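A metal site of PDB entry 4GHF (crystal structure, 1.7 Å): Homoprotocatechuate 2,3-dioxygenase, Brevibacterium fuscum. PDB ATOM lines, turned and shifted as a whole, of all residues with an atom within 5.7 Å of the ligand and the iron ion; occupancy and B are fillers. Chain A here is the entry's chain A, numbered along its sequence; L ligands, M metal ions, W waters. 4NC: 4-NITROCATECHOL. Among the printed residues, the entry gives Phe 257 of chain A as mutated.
O of Arg 293 sits at hydrogen-bond distance from ND1 of His 248 (3.1 Å). The backbone carbonyl oxygen (O) of Arg 292 lies close to the backbone NH (N) of Gly 249, at 3.4 Å. A ring nitrogen (NE2) of His 248 lies within hydrogen-bond range of the side-chain carboxylate (OE2) of Glu 267 (2.7 Å). The backbone carbonyl oxygen (O) of Arg 243 lies within hydrogen-bond range of the backbone NH (N) of Phe 257. The backbone carbonyl oxygen (O) of His 155 lies within hydrogen-bond range of the backbone NH (N) of Ala 216, 2.8 Å away. A ring nitrogen (ND1) of His 155 sits close to a ring nitrogen (NE2) of His 200 (3.3 Å). The backbone carbonyl oxygen (O) of His 214 sits at hydrogen-bond distance from the backbone NH (N) of Asn 157, at 3.0 Å. The guanidinium group (NH2) of Arg 243 sits at hydrogen-bond distance from the backbone carbonyl oxygen (O) of Arg 293 (3.3 Å).
Water W1 lies within hydrogen-bond range of a ring nitrogen (NE2) of His 200 (2.8 Å), the side-chain amide nitrogen (ND2) of Asn 157 (2.9 Å) and the indole nitrogen (NE1) of Trp 192 (3.4 Å).
The guanidinium group (NH1) of Arg 243 is in hydrogen-bond range of an oxygen (O10) of the ligand. O10 of the ligand sits at hydrogen-bond distance from NH1 of Arg 293 (3.1 Å). A ring nitrogen (NE2) of His 200 sits close to an oxygen (O7) of the ligand (3.2 Å). O11 of the ligand is in hydrogen-bond range of ND1 of His 248, at 3.2 Å.
The backbone carbonyl oxygen (O) of Arg 292 lies close to an oxygen (O11) of the ligand. Residues that only touch the ligand: Trp 192, Val 250, Ser 251, Phe 257 and Tyr 269. Hydrophobic or aromatic side chains that line the ligand: His 155, Trp 192, His 200, His 214, His 248, Val 250, Phe 257 and Tyr 269. Along chain A the residues within 4 Å of the ligand span positions 155 to 293.
The iron ion is bound by an oxygen (O8) of the ligand (2.1 Å), the side-chain carboxylate (OE1) of Glu 267 (2.1 Å), an oxygen (O7) of the ligand (2.1 Å), a ring nitrogen (NE2) of His 214 (2.2 Å), a ring nitrogen (NE2) of His 155 (2.2 Å) and water W1 (2.4 Å). The iron ion has six donor atoms within binding distance.
Residues that only touch the iron ion: His 200. Four residues have an atom within 4 Å of the iron ion: His 155, His 200, His 214 and Glu 267.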
ATOM      1  N   HIS A 155      -6.756 -23.745 -21.749  1.00  0.00           N
ATOM      2  CA  HIS A 155      -7.974 -23.905 -20.936  1.00  0.00           C
ATOM      3  C   HIS A 155      -8.713 -22.634 -20.661  1.00  0.00           C
ATOM      4  O   HIS A 155      -8.232 -21.521 -20.960  1.00  0.00           O
ATOM      5  CB  HIS A 155      -7.594 -24.543 -19.615  1.00  0.00           C
ATOM      6  CG  HIS A 155      -6.676 -23.676 -18.751  1.00  0.00           C
ATOM      7  ND1 HIS A 155      -5.324 -23.824 -18.739  1.00  0.00           N
ATOM      8  CD2 HIS A 155      -6.982 -22.733 -17.779  1.00  0.00           C
ATOM      9  CE1 HIS A 155      -4.796 -22.958 -17.828  1.00  0.00           C
ATOM     10  NE2 HIS A 155      -5.804 -22.279 -17.259  1.00  0.00           N
ATOM     11  N   ASN A 157     -11.123 -20.919 -17.296  1.00  0.00           N
ATOM     12  CA  ASN A 157     -11.375 -21.045 -15.850  1.00  0.00           C
ATOM     13  C   ASN A 157     -12.611 -20.233 -15.538  1.00  0.00           C
ATOM     14  O   ASN A 157     -12.702 -19.062 -15.876  1.00  0.00           O
ATOM     15  CB  ASN A 157     -10.168 -20.551 -15.022  1.00  0.00           C
ATOM     16  CG  ASN A 157     -10.333 -20.769 -13.555  1.00  0.00           C
ATOM     17  OD1 ASN A 157     -11.309 -20.321 -12.953  1.00  0.00           O
ATOM     18  ND2 ASN A 157      -9.333 -21.417 -12.940  1.00  0.00           N
ATOM     19  N   ILE A 181      -8.796 -27.933  -4.501  1.00  0.00           N
ATOM     20  CA  ILE A 181      -8.429 -27.230  -3.266  1.00  0.00           C
ATOM     21  C   ILE A 181      -9.599 -27.346  -2.326  1.00  0.00           C
ATOM     22  O   ILE A 181     -10.727 -26.998  -2.668  1.00  0.00           O
ATOM     23  CB  ILE A 181      -8.051 -25.743  -3.495  1.00  0.00           C
ATOM     24  CG1 ILE A 181      -6.907 -25.641  -4.459  1.00  0.00           C
ATOM     25  CG2 ILE A 181      -7.778 -25.041  -2.143  1.00  0.00           C
ATOM     26  CD1 ILE A 181      -6.466 -24.199  -4.829  1.00  0.00           C
ATOM     27  N   TRP A 192      -9.991 -28.580 -10.988  1.00  0.00           N
ATOM     28  CA  TRP A 192      -9.525 -28.575 -12.363  1.00  0.00           C
ATOM     29  C   TRP A 192      -9.924 -29.859 -13.029  1.00  0.00           C
ATOM     30  O   TRP A 192      -9.810 -30.925 -12.434  1.00  0.00           O
ATOM     31  CB  TRP A 192      -8.024 -28.480 -12.295  1.00  0.00           C
ATOM     32  CG  TRP A 192      -7.530 -27.108 -11.929  1.00  0.00           C
ATOM     33  CD1 TRP A 192      -7.009 -26.151 -12.776  1.00  0.00           C
ATOM     34  CD2 TRP A 192      -7.483 -26.513 -10.619  1.00  0.00           C
ATOM     35  NE1 TRP A 192      -6.660 -25.018 -12.103  1.00  0.00           N
ATOM     36  CE2 TRP A 192      -6.926 -25.157 -10.798  1.00  0.00           C
ATOM     37  CE3 TRP A 192      -7.815 -26.949  -9.346  1.00  0.00           C
ATOM     38  CZ2 TRP A 192      -6.740 -24.276  -9.736  1.00  0.00           C
ATOM     39  CZ3 TRP A 192      -7.646 -26.035  -8.281  1.00  0.00           C
ATOM     40  CH2 TRP A 192      -7.091 -24.746  -8.472  1.00  0.00           C
ATOM     41  N   HIS A 200      -6.020 -29.533 -17.310  1.00  0.00           N
ATOM     42  CA  HIS A 200      -7.354 -29.106 -17.504  1.00  0.00           C
ATOM     43  C   HIS A 200      -7.685 -28.533 -18.864  1.00  0.00           C
ATOM     44  O   HIS A 200      -6.814 -28.075 -19.596  1.00  0.00           O
ATOM     45  CB  HIS A 200      -7.834 -28.147 -16.442  1.00  0.00           C
ATOM     46  CG  HIS A 200      -6.965 -26.925 -16.236  1.00  0.00           C
ATOM     47  ND1 HIS A 200      -5.617 -26.941 -16.263  1.00  0.00           N
ATOM     48  CD2 HIS A 200      -7.330 -25.622 -15.920  1.00  0.00           C
ATOM     49  CE1 HIS A 200      -5.154 -25.689 -15.956  1.00  0.00           C
ATOM     50  NE2 HIS A 200      -6.213 -24.906 -15.739  1.00  0.00           N
ATOM     51  N   HIS A 214     -10.520 -16.520 -16.527  1.00  0.00           N
ATOM     52  CA  HIS A 214      -9.487 -16.294 -17.530  1.00  0.00           C
ATOM     53  C   HIS A 214      -9.572 -17.293 -18.635  1.00  0.00           C
ATOM     54  O   HIS A 214     -10.227 -18.303 -18.515  1.00  0.00           O
ATOM     55  CB  HIS A 214      -8.087 -16.282 -16.914  1.00  0.00           C
ATOM     56  CG  HIS A 214      -7.689 -17.551 -16.188  1.00  0.00           C
ATOM     57  ND1 HIS A 214      -7.870 -17.720 -14.862  1.00  0.00           N
ATOM     58  CD2 HIS A 214      -7.013 -18.689 -16.633  1.00  0.00           C
ATOM     59  CE1 HIS A 214      -7.392 -18.904 -14.479  1.00  0.00           C
ATOM     60  NE2 HIS A 214      -6.850 -19.503 -15.551  1.00  0.00           N
ATOM     61  N   ALA A 216      -6.540 -19.287 -21.021  1.00  0.00           N
ATOM     62  CA  ALA A 216      -5.117 -19.572 -20.884  1.00  0.00           C
ATOM     63  C   ALA A 216      -4.504 -20.025 -22.201  1.00  0.00           C
ATOM     64  O   ALA A 216      -5.100 -20.877 -22.896  1.00  0.00           O
ATOM     65  CB  ALA A 216      -4.911 -20.624 -19.804  1.00  0.00           C
ATOM     66  N   ARG A 243      -0.399 -10.745 -11.942  1.00  0.00           N
ATOM     67  CA  ARG A 243       0.134 -11.739 -11.030  1.00  0.00           C
ATOM     68  C   ARG A 243       1.138 -12.584 -11.763  1.00  0.00           C
ATOM     69  O   ARG A 243       0.944 -12.975 -12.900  1.00  0.00           O
ATOM     70  CB  ARG A 243      -1.017 -12.576 -10.450  1.00  0.00           C
ATOM     71  CG  ARG A 243      -0.598 -13.789  -9.666  1.00  0.00           C
ATOM     72  CD  ARG A 243      -1.721 -14.540  -8.941  1.00  0.00           C
ATOM     73  NE  ARG A 243      -1.106 -15.805  -8.507  1.00  0.00           N
ATOM     74  CZ  ARG A 243      -1.622 -17.023  -8.657  1.00  0.00           C
ATOM     75  NH1 ARG A 243      -2.875 -17.220  -9.046  1.00  0.00           N
ATOM     76  NH2 ARG A 243      -0.915 -18.058  -8.302  1.00  0.00           N
ATOM     77  N   HIS A 248       3.057 -22.587 -10.521  1.00  0.00           N
ATOM     78  CA  HIS A 248       1.833 -22.977  -9.808  1.00  0.00           C
ATOM     79  C   HIS A 248       2.126 -24.209  -8.951  1.00  0.00           C
ATOM     80  O   HIS A 248       3.002 -25.052  -9.295  1.00  0.00           O
ATOM     81  CB  HIS A 248       0.724 -23.385 -10.767  1.00  0.00           C
ATOM     82  CG  HIS A 248      -0.002 -22.254 -11.427  1.00  0.00           C
ATOM     83  ND1 HIS A 248      -0.632 -21.251 -10.716  1.00  0.00           N
ATOM     84  CD2 HIS A 248      -0.321 -22.064 -12.762  1.00  0.00           C
ATOM     85  CE1 HIS A 248      -1.263 -20.444 -11.607  1.00  0.00           C
ATOM     86  NE2 HIS A 248      -1.070 -20.948 -12.849  1.00  0.00           N
ATOM     87  N   GLY A 249       1.477 -24.332  -7.798  1.00  0.00           N
ATOM     88  CA  GLY A 249       1.422 -25.590  -7.058  1.00  0.00           C
ATOM     89  C   GLY A 249       0.512 -26.528  -7.810  1.00  0.00           C
ATOM     90  O   GLY A 249       0.952 -27.478  -8.395  1.00  0.00           O
ATOM     91  N   VAL A 250      -0.782 -26.249  -7.772  1.00  0.00           N
ATOM     92  CA  VAL A 250      -1.725 -26.960  -8.590  1.00  0.00           C
ATOM     93  C   VAL A 250      -1.328 -26.825 -10.071  1.00  0.00           C
ATOM     94  O   VAL A 250      -1.046 -25.721 -10.562  1.00  0.00           O
ATOM     95  CB  VAL A 250      -3.131 -26.301  -8.439  1.00  0.00           C
ATOM     96  CG1 VAL A 250      -4.135 -26.891  -9.474  1.00  0.00           C
ATOM     97  CG2 VAL A 250      -3.641 -26.431  -6.996  1.00  0.00           C
ATOM     98  N   SER A 251      -1.247 -27.940 -10.767  1.00  0.00           N
ATOM     99  CA  SER A 251      -0.847 -28.034 -12.201  1.00  0.00           C
ATOM    100  C   SER A 251       0.658 -28.116 -12.450  1.00  0.00           C
ATOM    101  O   SER A 251       1.062 -28.622 -13.484  1.00  0.00           O
ATOM    102  CB  SER A 251      -1.438 -26.968 -13.123  1.00  0.00           C
ATOM    103  OG  SER A 251      -0.716 -25.729 -13.054  1.00  0.00           O
ATOM    104  N   PHE A 257      -0.289 -13.996 -15.283  1.00  0.00           N
ATOM    105  CA  PHE A 257      -1.646 -13.370 -15.501  1.00  0.00           C
ATOM    106  C   PHE A 257      -1.518 -11.896 -15.887  1.00  0.00           C
ATOM    107  O   PHE A 257      -0.947 -11.059 -15.130  1.00  0.00           O
ATOM    108  CB  PHE A 257      -2.516 -13.491 -14.236  1.00  0.00           C
ATOM    109  CG  PHE A 257      -2.909 -14.918 -13.887  1.00  0.00           C
ATOM    110  CD1 PHE A 257      -3.890 -15.569 -14.584  1.00  0.00           C
ATOM    111  CD2 PHE A 257      -2.206 -15.621 -12.969  1.00  0.00           C
ATOM    112  CE1 PHE A 257      -4.215 -16.909 -14.309  1.00  0.00           C
ATOM    113  CE2 PHE A 257      -2.548 -16.977 -12.687  1.00  0.00           C
ATOM    114  CZ  PHE A 257      -3.513 -17.605 -13.367  1.00  0.00           C
ATOM    115  N   GLU A 267      -4.226 -15.838 -19.060  1.00  0.00           N
ATOM    116  CA  GLU A 267      -3.081 -16.552 -18.507  1.00  0.00           C
ATOM    117  C   GLU A 267      -2.181 -17.069 -19.603  1.00  0.00           C
ATOM    118  O   GLU A 267      -2.651 -17.590 -20.634  1.00  0.00           O
ATOM    119  CB  GLU A 267      -3.568 -17.743 -17.660  1.00  0.00           C
ATOM    120  CG  GLU A 267      -2.474 -18.373 -16.836  1.00  0.00           C
ATOM    121  CD  GLU A 267      -2.927 -19.608 -16.073  1.00  0.00           C
ATOM    122  OE1 GLU A 267      -4.036 -20.062 -16.356  1.00  0.00           O
ATOM    123  OE2 GLU A 267      -2.163 -20.148 -15.222  1.00  0.00           O
ATOM    124  N   TYR A 269       0.834 -19.916 -19.876  1.00  0.00           N
ATOM    125  CA  TYR A 269       0.975 -21.164 -19.113  1.00  0.00           C
ATOM    126  C   TYR A 269       1.939 -22.098 -19.829  1.00  0.00           C
ATOM    127  O   TYR A 269       1.981 -22.146 -21.065  1.00  0.00           O
ATOM    128  CB  TYR A 269      -0.452 -21.746 -19.082  1.00  0.00           C
ATOM    129  CG  TYR A 269      -0.750 -22.983 -18.338  1.00  0.00           C
ATOM    130  CD1 TYR A 269      -1.193 -22.946 -16.994  1.00  0.00           C
ATOM    131  CD2 TYR A 269      -0.732 -24.229 -18.987  1.00  0.00           C
ATOM    132  CE1 TYR A 269      -1.565 -24.086 -16.313  1.00  0.00           C
ATOM    133  CE2 TYR A 269      -1.108 -25.381 -18.300  1.00  0.00           C
ATOM    134  CZ  TYR A 269      -1.523 -25.287 -16.960  1.00  0.00           C
ATOM    135  OH  TYR A 269      -1.895 -26.430 -16.313  1.00  0.00           O
ATOM    136  N   ARG A 292       0.192 -23.625  -2.700  1.00  0.00           N
ATOM    137  CA  ARG A 292      -0.790 -24.305  -3.546  1.00  0.00           C
ATOM    138  C   ARG A 292      -1.043 -23.546  -4.839  1.00  0.00           C
ATOM    139  O   ARG A 292      -1.313 -24.171  -5.877  1.00  0.00           O
ATOM    140  CB  ARG A 292      -2.133 -24.422  -2.799  1.00  0.00           C
ATOM    141  CG  ARG A 292      -2.926 -23.178  -2.740  1.00  0.00           C
ATOM    142  CD  ARG A 292      -4.055 -23.207  -1.689  1.00  0.00           C
ATOM    143  NE  ARG A 292      -4.724 -21.938  -1.765  1.00  0.00           N
ATOM    144  CZ  ARG A 292      -4.249 -20.792  -1.273  1.00  0.00           C
ATOM    145  NH1 ARG A 292      -3.147 -20.767  -0.553  1.00  0.00           N
ATOM    146  NH2 ARG A 292      -4.914 -19.667  -1.442  1.00  0.00           N
ATOM    147  N   ARG A 293      -0.977 -22.239  -4.796  1.00  0.00           N
ATOM    148  CA  ARG A 293      -1.279 -21.459  -5.980  1.00  0.00           C
ATOM    149  C   ARG A 293       0.016 -20.930  -6.568  1.00  0.00           C
ATOM    150  O   ARG A 293       0.215 -21.060  -7.755  1.00  0.00           O
ATOM    151  CB  ARG A 293      -2.217 -20.338  -5.692  1.00  0.00           C
ATOM    152  CG  ARG A 293      -3.666 -20.819  -5.550  1.00  0.00           C
ATOM    153  CD  ARG A 293      -4.663 -19.717  -5.708  1.00  0.00           C
ATOM    154  NE  ARG A 293      -6.016 -20.274  -5.625  1.00  0.00           N
ATOM    155  CZ  ARG A 293      -6.719 -20.830  -6.598  1.00  0.00           C
ATOM    156  NH1 ARG A 293      -6.245 -20.964  -7.831  1.00  0.00           N
ATOM    157  NH2 ARG A 293      -7.959 -21.213  -6.350  1.00  0.00           N
ATOM    158  N   ASP A 294       0.837 -20.259  -5.781  1.00  0.00           N
ATOM    159  CA  ASP A 294       2.197 -19.964  -6.181  1.00  0.00           C
ATOM    160  C   ASP A 294       3.128 -20.865  -5.369  1.00  0.00           C
ATOM    161  O   ASP A 294       3.204 -20.715  -4.143  1.00  0.00           O
ATOM    162  CB  ASP A 294       2.563 -18.468  -5.990  1.00  0.00           C
ATOM    163  CG  ASP A 294       3.930 -18.133  -6.632  1.00  0.00           C
ATOM    164  OD1 ASP A 294       4.968 -18.138  -5.883  1.00  0.00           O
ATOM    165  OD2 ASP A 294       3.948 -17.906  -7.866  1.00  0.00           O
ATOM    166  N   TRP A 304      -7.073 -10.884  -8.004  1.00  0.00           N
ATOM    167  CA  TRP A 304      -7.140 -12.166  -8.645  1.00  0.00           C
ATOM    168  C   TRP A 304      -8.332 -12.969  -8.144  1.00  0.00           C
ATOM    169  O   TRP A 304      -8.975 -13.716  -8.903  1.00  0.00           O
ATOM    170  CB  TRP A 304      -5.778 -12.881  -8.459  1.00  0.00           C
ATOM    171  CG  TRP A 304      -5.616 -14.056  -9.367  1.00  0.00           C
ATOM    172  CD1 TRP A 304      -5.084 -14.065 -10.615  1.00  0.00           C
ATOM    173  CD2 TRP A 304      -6.099 -15.412  -9.132  1.00  0.00           C
ATOM    174  NE1 TRP A 304      -5.158 -15.319 -11.171  1.00  0.00           N
ATOM    175  CE2 TRP A 304      -5.763 -16.169 -10.320  1.00  0.00           C
ATOM    176  CE3 TRP A 304      -6.722 -16.044  -8.085  1.00  0.00           C
ATOM    177  CZ2 TRP A 304      -6.102 -17.529 -10.455  1.00  0.00           C
ATOM    178  CZ3 TRP A 304      -7.039 -17.404  -8.223  1.00  0.00           C
ATOM    179  CH2 TRP A 304      -6.705 -18.127  -9.398  1.00  0.00           C
HETATM  180  C1  4NC L   1      -4.066 -22.580 -13.415  1.00  0.00           C
HETATM  181  C2  4NC L   1      -4.649 -21.417 -12.738  1.00  0.00           C
HETATM  182  C3  4NC L   1      -4.566 -21.312 -11.369  1.00  0.00           C
HETATM  183  C4  4NC L   1      -3.882 -22.303 -10.655  1.00  0.00           C
HETATM  184  C5  4NC L   1      -3.342 -23.418 -11.288  1.00  0.00           C
HETATM  185  C6  4NC L   1      -3.429 -23.586 -12.679  1.00  0.00           C
HETATM  186  O7  4NC L   1      -4.136 -22.702 -14.749  1.00  0.00           O
HETATM  187  O8  4NC L   1      -5.242 -20.455 -13.409  1.00  0.00           O
HETATM  188  N9  4NC L   1      -3.580 -22.042  -9.363  1.00  0.00           N
HETATM  189  O10 4NC L   1      -3.389 -20.548  -9.015  1.00  0.00           O
HETATM  190  O11 4NC L   1      -2.638 -22.842  -8.763  1.00  0.00           O
HETATM  191 FE    FE M   1      -5.494 -21.184 -15.348  1.00  0.00          FE
HETATM  192  O   HOH W   1      -7.196 -22.580 -14.429  1.00  0.00           O
